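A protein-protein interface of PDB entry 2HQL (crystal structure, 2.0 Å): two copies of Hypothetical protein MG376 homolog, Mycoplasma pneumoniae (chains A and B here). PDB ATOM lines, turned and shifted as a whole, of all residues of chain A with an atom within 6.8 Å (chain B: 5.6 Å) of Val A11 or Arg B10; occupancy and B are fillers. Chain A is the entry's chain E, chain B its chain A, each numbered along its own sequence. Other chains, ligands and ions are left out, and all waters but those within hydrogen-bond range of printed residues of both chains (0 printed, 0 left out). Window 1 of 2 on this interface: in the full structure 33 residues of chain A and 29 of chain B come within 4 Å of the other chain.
The backbone carbonyl oxygen (O) of Arg B10 sits at hydrogen-bond distance from the backbone NH (N) of Phe A12 (2.8 Å). The backbone carbonyl oxygen of Phe B12 sits close to the backbone NH of Asn A9 (3.5 Å). The backbone NH of Phe B12 is in hydrogen-bond range of the backbone carbonyl oxygen of Arg A10 (2.8 Å).
OD1 of Asn B9 lies within hydrogen-bond range of N of Leu B76 (2.8 Å). The guanidinium group of Arg B10 is in salt-bridge range of the side-chain carboxylate of Glu B73 (3.3 Å). The backbone carbonyl oxygen (O) of Val B11 sits at hydrogen-bond distance from the backbone NH (N) of Gly B74, at 2.6 Å. NE of Arg A10 lies within salt-bridge range of OE2 of Glu A73. N of Val A11 sits at hydrogen-bond distance from O of Gly A74, at 2.8 Å. The backbone NH of Ile A72 sits at hydrogen-bond distance from the backbone carbonyl oxygen of Leu A13, 2.9 Å away.
O of Arg A10 touches O of Arg B10, at 3.9 Å. O of Arg A10 touches CA of Val B11 (3.3 Å). O of Arg B10 touches CA of Val A11, 3.4 Å away. Val B11 touches Val A11. Phe A12 touches Leu B8 (O to O, 3.6 Å). Phe A12 touches Asn B9 (O to CA, 3.3 Å). Leu B8 touches Leu A13. ND2 of Asn B9 touches CD1 of Leu A13 (3.8 Å). Leu B76 touches Leu A76 (CD2 to CD1, 3.8 Å). Ile A91 touches Leu B76 (CD1 to CD2, 3.8 Å).
Of the printed residues of chain B, Asn A9 touches Phe B12. Val A11 touches just these residues of chain B: Arg B10 (3.4 Å) and Val B11 (3.7 Å). Of the printed residues of chain B, Phe A12 touches Leu B8 (3.6 Å), Asn B9 (3.3 Å) and Arg B10 (2.8 Å). Arg B10 touches just these residues of chain A: Arg A10, Val A11 and Phe A12. Of the printed residues of chain A, Phe B12 touches Asn A9 (3.1 Å) and Arg A10 (2.8 Å). The nearest residue of chain B that does not touch Val A11 is Leu B76 (4.4 Å).
Of the 9 printed residues of chain B, 6 touch a printed residue of chain A. Hydrophobic or aromatic side chains of chain B within 4 Å of the printed part of chain A: Leu B8, Val B11 and Leu B76. Printed residues of chain A that touch a printed residue of chain B: Asn A9, Arg A10, Val A11, Phe A12, Leu A13, Leu A76 and Ile A91. Hydrophobic or aromatic side chains of chain A within 4 Å of the printed part of chain B: Val A11, Phe A12, Leu A13, Leu A76 and Ile A91. Among the printed residues, 13 pairs touch across the chains. Among the printed residues, no Asp or Glu carboxylate lies within 4 Å of a Lys or Arg side-chain nitrogen of the other chain.
Asn A9 touches Phe B12, and with the chains exchanged Phe A12 touches Asn B9. Arg B10 touches its own counterpart, Arg A10. Arg A10 touches Val B11, and with the chains exchanged Val A11 touches Arg B10. Val A11 touches its own counterpart, Val B11. Positions printed for both chains: 9, 10, 11, 12, 73, 74, 75 and 76.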
ATOM      1  N   ASN A   9     -11.676  16.834  22.736  1.00  0.00           N
ATOM      2  CA  ASN A   9     -10.739  15.934  22.089  1.00  0.00           C
ATOM      3  C   ASN A   9     -10.304  16.570  20.771  1.00  0.00           C
ATOM      4  O   ASN A   9     -11.043  16.546  19.786  1.00  0.00           O
ATOM      5  CB  ASN A   9     -11.398  14.574  21.815  1.00  0.00           C
ATOM      6  CG  ASN A   9     -10.419  13.541  21.269  1.00  0.00           C
ATOM      7  OD1 ASN A   9      -9.535  13.865  20.475  1.00  0.00           O
ATOM      8  ND2 ASN A   9     -10.587  12.285  21.683  1.00  0.00           N
ATOM      9  N   ARG A  10      -9.110  17.153  20.767  1.00  0.00           N
ATOM     10  CA  ARG A  10      -8.548  17.789  19.574  1.00  0.00           C
ATOM     11  C   ARG A  10      -7.062  17.519  19.569  1.00  0.00           C
ATOM     12  O   ARG A  10      -6.395  17.678  20.582  1.00  0.00           O
ATOM     13  CB  ARG A  10      -8.769  19.310  19.586  1.00  0.00           C
ATOM     14  CG  ARG A  10      -9.822  19.804  18.599  1.00  0.00           C
ATOM     15  CD  ARG A  10      -9.498  19.328  17.195  1.00  0.00           C
ATOM     16  NE  ARG A  10     -10.682  19.226  16.345  1.00  0.00           N
ATOM     17  CZ  ARG A  10     -11.816  18.610  16.685  1.00  0.00           C
ATOM     18  NH1 ARG A  10     -11.951  18.034  17.876  1.00  0.00           N
ATOM     19  NH2 ARG A  10     -12.815  18.534  15.810  1.00  0.00           N
ATOM     20  N   VAL A  11      -6.546  17.085  18.432  1.00  0.00           N
ATOM     21  CA  VAL A  11      -5.127  16.823  18.310  1.00  0.00           C
ATOM     22  C   VAL A  11      -4.630  17.533  17.076  1.00  0.00           C
ATOM     23  O   VAL A  11      -5.303  17.567  16.053  1.00  0.00           O
ATOM     24  CB  VAL A  11      -4.810  15.306  18.171  1.00  0.00           C
ATOM     25  CG1 VAL A  11      -3.338  15.108  17.843  1.00  0.00           C
ATOM     26  CG2 VAL A  11      -5.134  14.577  19.474  1.00  0.00           C
ATOM     27  N   PHE A  12      -3.462  18.140  17.196  1.00  0.00           N
ATOM     28  CA  PHE A  12      -2.827  18.821  16.081  1.00  0.00           C
ATOM     29  C   PHE A  12      -1.480  18.147  16.051  1.00  0.00           C
ATOM     30  O   PHE A  12      -0.680  18.305  16.977  1.00  0.00           O
ATOM     31  CB  PHE A  12      -2.724  20.320  16.358  1.00  0.00           C
ATOM     32  CG  PHE A  12      -4.052  21.017  16.309  1.00  0.00           C
ATOM     33  CD1 PHE A  12      -4.607  21.390  15.092  1.00  0.00           C
ATOM     34  CD2 PHE A  12      -4.796  21.214  17.469  1.00  0.00           C
ATOM     35  CE1 PHE A  12      -5.877  21.945  15.028  1.00  0.00           C
ATOM     36  CE2 PHE A  12      -6.077  21.771  17.411  1.00  0.00           C
ATOM     37  CZ  PHE A  12      -6.618  22.134  16.189  1.00  0.00           C
ATOM     38  N   LEU A  13      -1.257  17.355  15.006  1.00  0.00           N
ATOM     39  CA  LEU A  13      -0.023  16.604  14.877  1.00  0.00           C
ATOM     40  C   LEU A  13       0.603  16.727  13.501  1.00  0.00           C
ATOM     41  O   LEU A  13      -0.082  16.759  12.474  1.00  0.00           O
ATOM     42  CB  LEU A  13      -0.289  15.125  15.207  1.00  0.00           C
ATOM     43  CG  LEU A  13       0.840  14.139  15.554  1.00  0.00           C
ATOM     44  CD1 LEU A  13       1.745  14.686  16.640  1.00  0.00           C
ATOM     45  CD2 LEU A  13       0.208  12.822  16.021  1.00  0.00           C
ATOM     46  N   ILE A  72      -1.768  17.228  10.209  1.00  0.00           N
ATOM     47  CA  ILE A  72      -3.220  17.075  10.242  1.00  0.00           C
ATOM     48  C   ILE A  72      -3.912  17.639  11.467  1.00  0.00           C
ATOM     49  O   ILE A  72      -3.297  18.263  12.333  1.00  0.00           O
ATOM     50  CB  ILE A  72      -3.622  15.589  10.189  1.00  0.00           C
ATOM     51  CG1 ILE A  72      -3.171  14.890  11.469  1.00  0.00           C
ATOM     52  CG2 ILE A  72      -3.009  14.924   8.966  1.00  0.00           C
ATOM     53  CD1 ILE A  72      -4.146  13.854  11.991  1.00  0.00           C
ATOM     54  N   GLU A  73      -5.219  17.400  11.514  1.00  0.00           N
ATOM     55  CA  GLU A  73      -6.059  17.779  12.638  1.00  0.00           C
ATOM     56  C   GLU A  73      -6.996  16.602  12.821  1.00  0.00           C
ATOM     57  O   GLU A  73      -7.422  15.998  11.845  1.00  0.00           O
ATOM     58  CB  GLU A  73      -6.863  19.037  12.340  1.00  0.00           C
ATOM     59  CG  GLU A  73      -7.526  19.622  13.577  1.00  0.00           C
ATOM     60  CD  GLU A  73      -8.913  20.151  13.296  1.00  0.00           C
ATOM     61  OE1 GLU A  73      -9.079  20.849  12.274  1.00  0.00           O
ATOM     62  OE2 GLU A  73      -9.835  19.878  14.094  1.00  0.00           O
ATOM     63  N   GLY A  74      -7.305  16.269  14.067  1.00  0.00           N
ATOM     64  CA  GLY A  74      -8.189  15.149  14.313  1.00  0.00           C
ATOM     65  C   GLY A  74      -8.457  14.888  15.779  1.00  0.00           C
ATOM     66  O   GLY A  74      -8.200  15.737  16.633  1.00  0.00           O
ATOM     67  N   ILE A  75      -8.979  13.698  16.062  1.00  0.00           N
ATOM     68  CA  ILE A  75      -9.338  13.294  17.417  1.00  0.00           C
ATOM     69  C   ILE A  75      -8.599  12.023  17.836  1.00  0.00           C
ATOM     70  O   ILE A  75      -8.295  11.155  17.013  1.00  0.00           O
ATOM     71  CB  ILE A  75     -10.861  13.038  17.521  1.00  0.00           C
ATOM     72  CG1 ILE A  75     -11.304  12.124  16.382  1.00  0.00           C
ATOM     73  CG2 ILE A  75     -11.620  14.358  17.463  1.00  0.00           C
ATOM     74  CD1 ILE A  75     -12.796  11.917  16.319  1.00  0.00           C
ATOM     75  N   LEU A  76      -8.309  11.924  19.126  1.00  0.00           N
ATOM     76  CA  LEU A  76      -7.618  10.765  19.669  1.00  0.00           C
ATOM     77  C   LEU A  76      -8.677   9.672  19.846  1.00  0.00           C
ATOM     78  O   LEU A  76      -9.797   9.952  20.294  1.00  0.00           O
ATOM     79  CB  LEU A  76      -6.975  11.140  21.015  1.00  0.00           C
ATOM     80  CG  LEU A  76      -5.771  10.360  21.548  1.00  0.00           C
ATOM     81  CD1 LEU A  76      -4.684  10.338  20.506  1.00  0.00           C
ATOM     82  CD2 LEU A  76      -5.251  11.016  22.819  1.00  0.00           C
ATOM     83  N   ILE A  91      -5.057   8.297  15.809  1.00  0.00           N
ATOM     84  CA  ILE A  91      -5.718   9.576  15.578  1.00  0.00           C
ATOM     85  C   ILE A  91      -6.540   9.451  14.307  1.00  0.00           C
ATOM     86  O   ILE A  91      -6.040   9.017  13.272  1.00  0.00           O
ATOM     87  CB  ILE A  91      -4.733  10.763  15.381  1.00  0.00           C
ATOM     88  CG1 ILE A  91      -3.941  11.038  16.659  1.00  0.00           C
ATOM     89  CG2 ILE A  91      -5.512  12.023  15.034  1.00  0.00           C
ATOM     90  CD1 ILE A  91      -2.704  10.188  16.807  1.00  0.00           C
ATOM     91  N   PHE A  97      -3.460  19.388   6.524  1.00  0.00           N
ATOM     92  CA  PHE A  97      -3.055  20.758   6.267  1.00  0.00           C
ATOM     93  C   PHE A  97      -2.153  20.879   5.052  1.00  0.00           C
ATOM     94  O   PHE A  97      -1.596  19.893   4.568  1.00  0.00           O
ATOM     95  CB  PHE A  97      -2.355  21.335   7.496  1.00  0.00           C
ATOM     96  CG  PHE A  97      -3.284  21.627   8.627  1.00  0.00           C
ATOM     97  CD1 PHE A  97      -4.254  22.612   8.499  1.00  0.00           C
ATOM     98  CD2 PHE A  97      -3.220  20.895   9.806  1.00  0.00           C
ATOM     99  CE1 PHE A  97      -5.153  22.869   9.522  1.00  0.00           C
ATOM    100  CE2 PHE A  97      -4.115  21.138  10.844  1.00  0.00           C
ATOM    101  CZ  PHE A  97      -5.086  22.129  10.703  1.00  0.00           C
ATOM    102  N   VAL A 104      -1.032  27.322  14.322  1.00  0.00           N
ATOM    103  CA  VAL A 104      -1.222  28.194  15.467  1.00  0.00           C
ATOM    104  C   VAL A 104      -2.650  28.179  16.020  1.00  0.00           C
ATOM    105  O   VAL A 104      -2.869  27.518  17.068  1.00  0.00           O
ATOM    106  CB  VAL A 104      -0.819  29.659  15.156  1.00  0.00           C
ATOM    107  CG1 VAL A 104      -0.816  30.474  16.428  1.00  0.00           C
ATOM    108  CG2 VAL A 104       0.562  29.704  14.512  1.00  0.00           C
ATOM    109  N   LEU B   8       4.698  20.444  15.230  1.00  0.00           N
ATOM    110  CA  LEU B   8       3.246  20.630  15.547  1.00  0.00           C
ATOM    111  C   LEU B   8       2.821  19.445  16.422  1.00  0.00           C
ATOM    112  O   LEU B   8       2.739  18.297  15.953  1.00  0.00           O
ATOM    113  CB  LEU B   8       2.316  20.684  14.322  1.00  0.00           C
ATOM    114  CG  LEU B   8       0.819  20.964  14.597  1.00  0.00           C
ATOM    115  CD1 LEU B   8       0.650  22.085  15.609  1.00  0.00           C
ATOM    116  CD2 LEU B   8       0.084  21.297  13.304  1.00  0.00           C
ATOM    117  N   ASN B   9       2.552  19.721  17.692  1.00  0.00           N
ATOM    118  CA  ASN B   9       2.154  18.680  18.632  1.00  0.00           C
ATOM    119  C   ASN B   9       1.389  19.250  19.822  1.00  0.00           C
ATOM    120  O   ASN B   9       1.989  19.595  20.841  1.00  0.00           O
ATOM    121  CB  ASN B   9       3.377  17.910  19.152  1.00  0.00           C
ATOM    122  CG  ASN B   9       2.994  16.602  19.828  1.00  0.00           C
ATOM    123  OD1 ASN B   9       1.939  16.497  20.447  1.00  0.00           O
ATOM    124  ND2 ASN B   9       3.854  15.604  19.715  1.00  0.00           N
ATOM    125  N   ARG B  10       0.069  19.346  19.684  1.00  0.00           N
ATOM    126  CA  ARG B  10      -0.788  19.842  20.755  1.00  0.00           C
ATOM    127  C   ARG B  10      -2.053  18.977  20.860  1.00  0.00           C
ATOM    128  O   ARG B  10      -2.640  18.587  19.848  1.00  0.00           O
ATOM    129  CB  ARG B  10      -1.138  21.308  20.509  1.00  0.00           C
ATOM    130  CG  ARG B  10       0.089  22.190  20.559  1.00  0.00           C
ATOM    131  CD  ARG B  10      -0.224  23.665  20.561  1.00  0.00           C
ATOM    132  NE  ARG B  10      -1.135  24.045  21.636  1.00  0.00           N
ATOM    133  CZ  ARG B  10      -1.387  25.305  21.979  1.00  0.00           C
ATOM    134  NH1 ARG B  10      -0.784  26.294  21.334  1.00  0.00           N
ATOM    135  NH2 ARG B  10      -2.259  25.578  22.941  1.00  0.00           N
ATOM    136  N   VAL B  11      -2.448  18.666  22.094  1.00  0.00           N
ATOM    137  CA  VAL B  11      -3.616  17.831  22.367  1.00  0.00           C
ATOM    138  C   VAL B  11      -4.481  18.475  23.443  1.00  0.00           C
ATOM    139  O   VAL B  11      -3.959  19.003  24.416  1.00  0.00           O
ATOM    140  CB  VAL B  11      -3.186  16.444  22.913  1.00  0.00           C
ATOM    141  CG1 VAL B  11      -4.378  15.503  23.001  1.00  0.00           C
ATOM    142  CG2 VAL B  11      -2.092  15.869  22.047  1.00  0.00           C
ATOM    143  N   PHE B  12      -5.797  18.425  23.264  1.00  0.00           N
ATOM    144  CA  PHE B  12      -6.752  18.945  24.241  1.00  0.00           C
ATOM    145  C   PHE B  12      -7.701  17.784  24.501  1.00  0.00           C
ATOM    146  O   PHE B  12      -8.309  17.241  23.573  1.00  0.00           O
ATOM    147  CB  PHE B  12      -7.506  20.138  23.670  1.00  0.00           C
ATOM    148  CG  PHE B  12      -6.629  21.310  23.396  1.00  0.00           C
ATOM    149  CD1 PHE B  12      -6.541  22.352  24.310  1.00  0.00           C
ATOM    150  CD2 PHE B  12      -5.864  21.362  22.234  1.00  0.00           C
ATOM    151  CE1 PHE B  12      -5.704  23.425  24.078  1.00  0.00           C
ATOM    152  CE2 PHE B  12      -5.015  22.437  21.989  1.00  0.00           C
ATOM    153  CZ  PHE B  12      -4.936  23.472  22.914  1.00  0.00           C
ATOM    154  N   GLU B  73      -4.411  20.326  28.358  1.00  0.00           N
ATOM    155  CA  GLU B  73      -3.765  20.705  27.112  1.00  0.00           C
ATOM    156  C   GLU B  73      -2.456  19.931  27.242  1.00  0.00           C
ATOM    157  O   GLU B  73      -1.798  19.997  28.276  1.00  0.00           O
ATOM    158  CB  GLU B  73      -3.477  22.203  27.053  1.00  0.00           C
ATOM    159  CG  GLU B  73      -3.166  22.693  25.641  1.00  0.00           C
ATOM    160  CD  GLU B  73      -1.707  23.040  25.415  1.00  0.00           C
ATOM    161  OE1 GLU B  73      -1.201  23.899  26.165  1.00  0.00           O
ATOM    162  OE2 GLU B  73      -1.073  22.472  24.488  1.00  0.00           O
ATOM    163  N   GLY B  74      -2.074  19.176  26.225  1.00  0.00           N
ATOM    164  CA  GLY B  74      -0.844  18.427  26.365  1.00  0.00           C
ATOM    165  C   GLY B  74      -0.153  18.121  25.065  1.00  0.00           C
ATOM    166  O   GLY B  74      -0.552  18.600  24.000  1.00  0.00           O
ATOM    167  N   ILE B  75       0.889  17.303  25.162  1.00  0.00           N
ATOM    168  CA  ILE B  75       1.684  16.913  24.006  1.00  0.00           C
ATOM    169  C   ILE B  75       1.650  15.391  23.850  1.00  0.00           C
ATOM    170  O   ILE B  75       1.973  14.645  24.774  1.00  0.00           O
ATOM    171  CB  ILE B  75       3.137  17.397  24.181  1.00  0.00           C
ATOM    172  CG1 ILE B  75       3.143  18.874  24.595  1.00  0.00           C
ATOM    173  CG2 ILE B  75       3.889  17.256  22.897  1.00  0.00           C
ATOM    174  CD1 ILE B  75       4.521  19.425  24.929  1.00  0.00           C
ATOM    175  N   LEU B  76       1.251  14.929  22.676  1.00  0.00           N
ATOM    176  CA  LEU B  76       1.178  13.496  22.436  1.00  0.00           C
ATOM    177  C   LEU B  76       2.563  12.850  22.281  1.00  0.00           C
ATOM    178  O   LEU B  76       3.331  13.200  21.380  1.00  0.00           O
ATOM    179  CB  LEU B  76       0.319  13.233  21.201  1.00  0.00           C
ATOM    180  CG  LEU B  76      -0.324  11.851  21.102  1.00  0.00           C
ATOM    181  CD1 LEU B  76      -1.134  11.554  22.355  1.00  0.00           C
ATOM    182  CD2 LEU B  76      -1.209  11.807  19.886  1.00  0.00           C
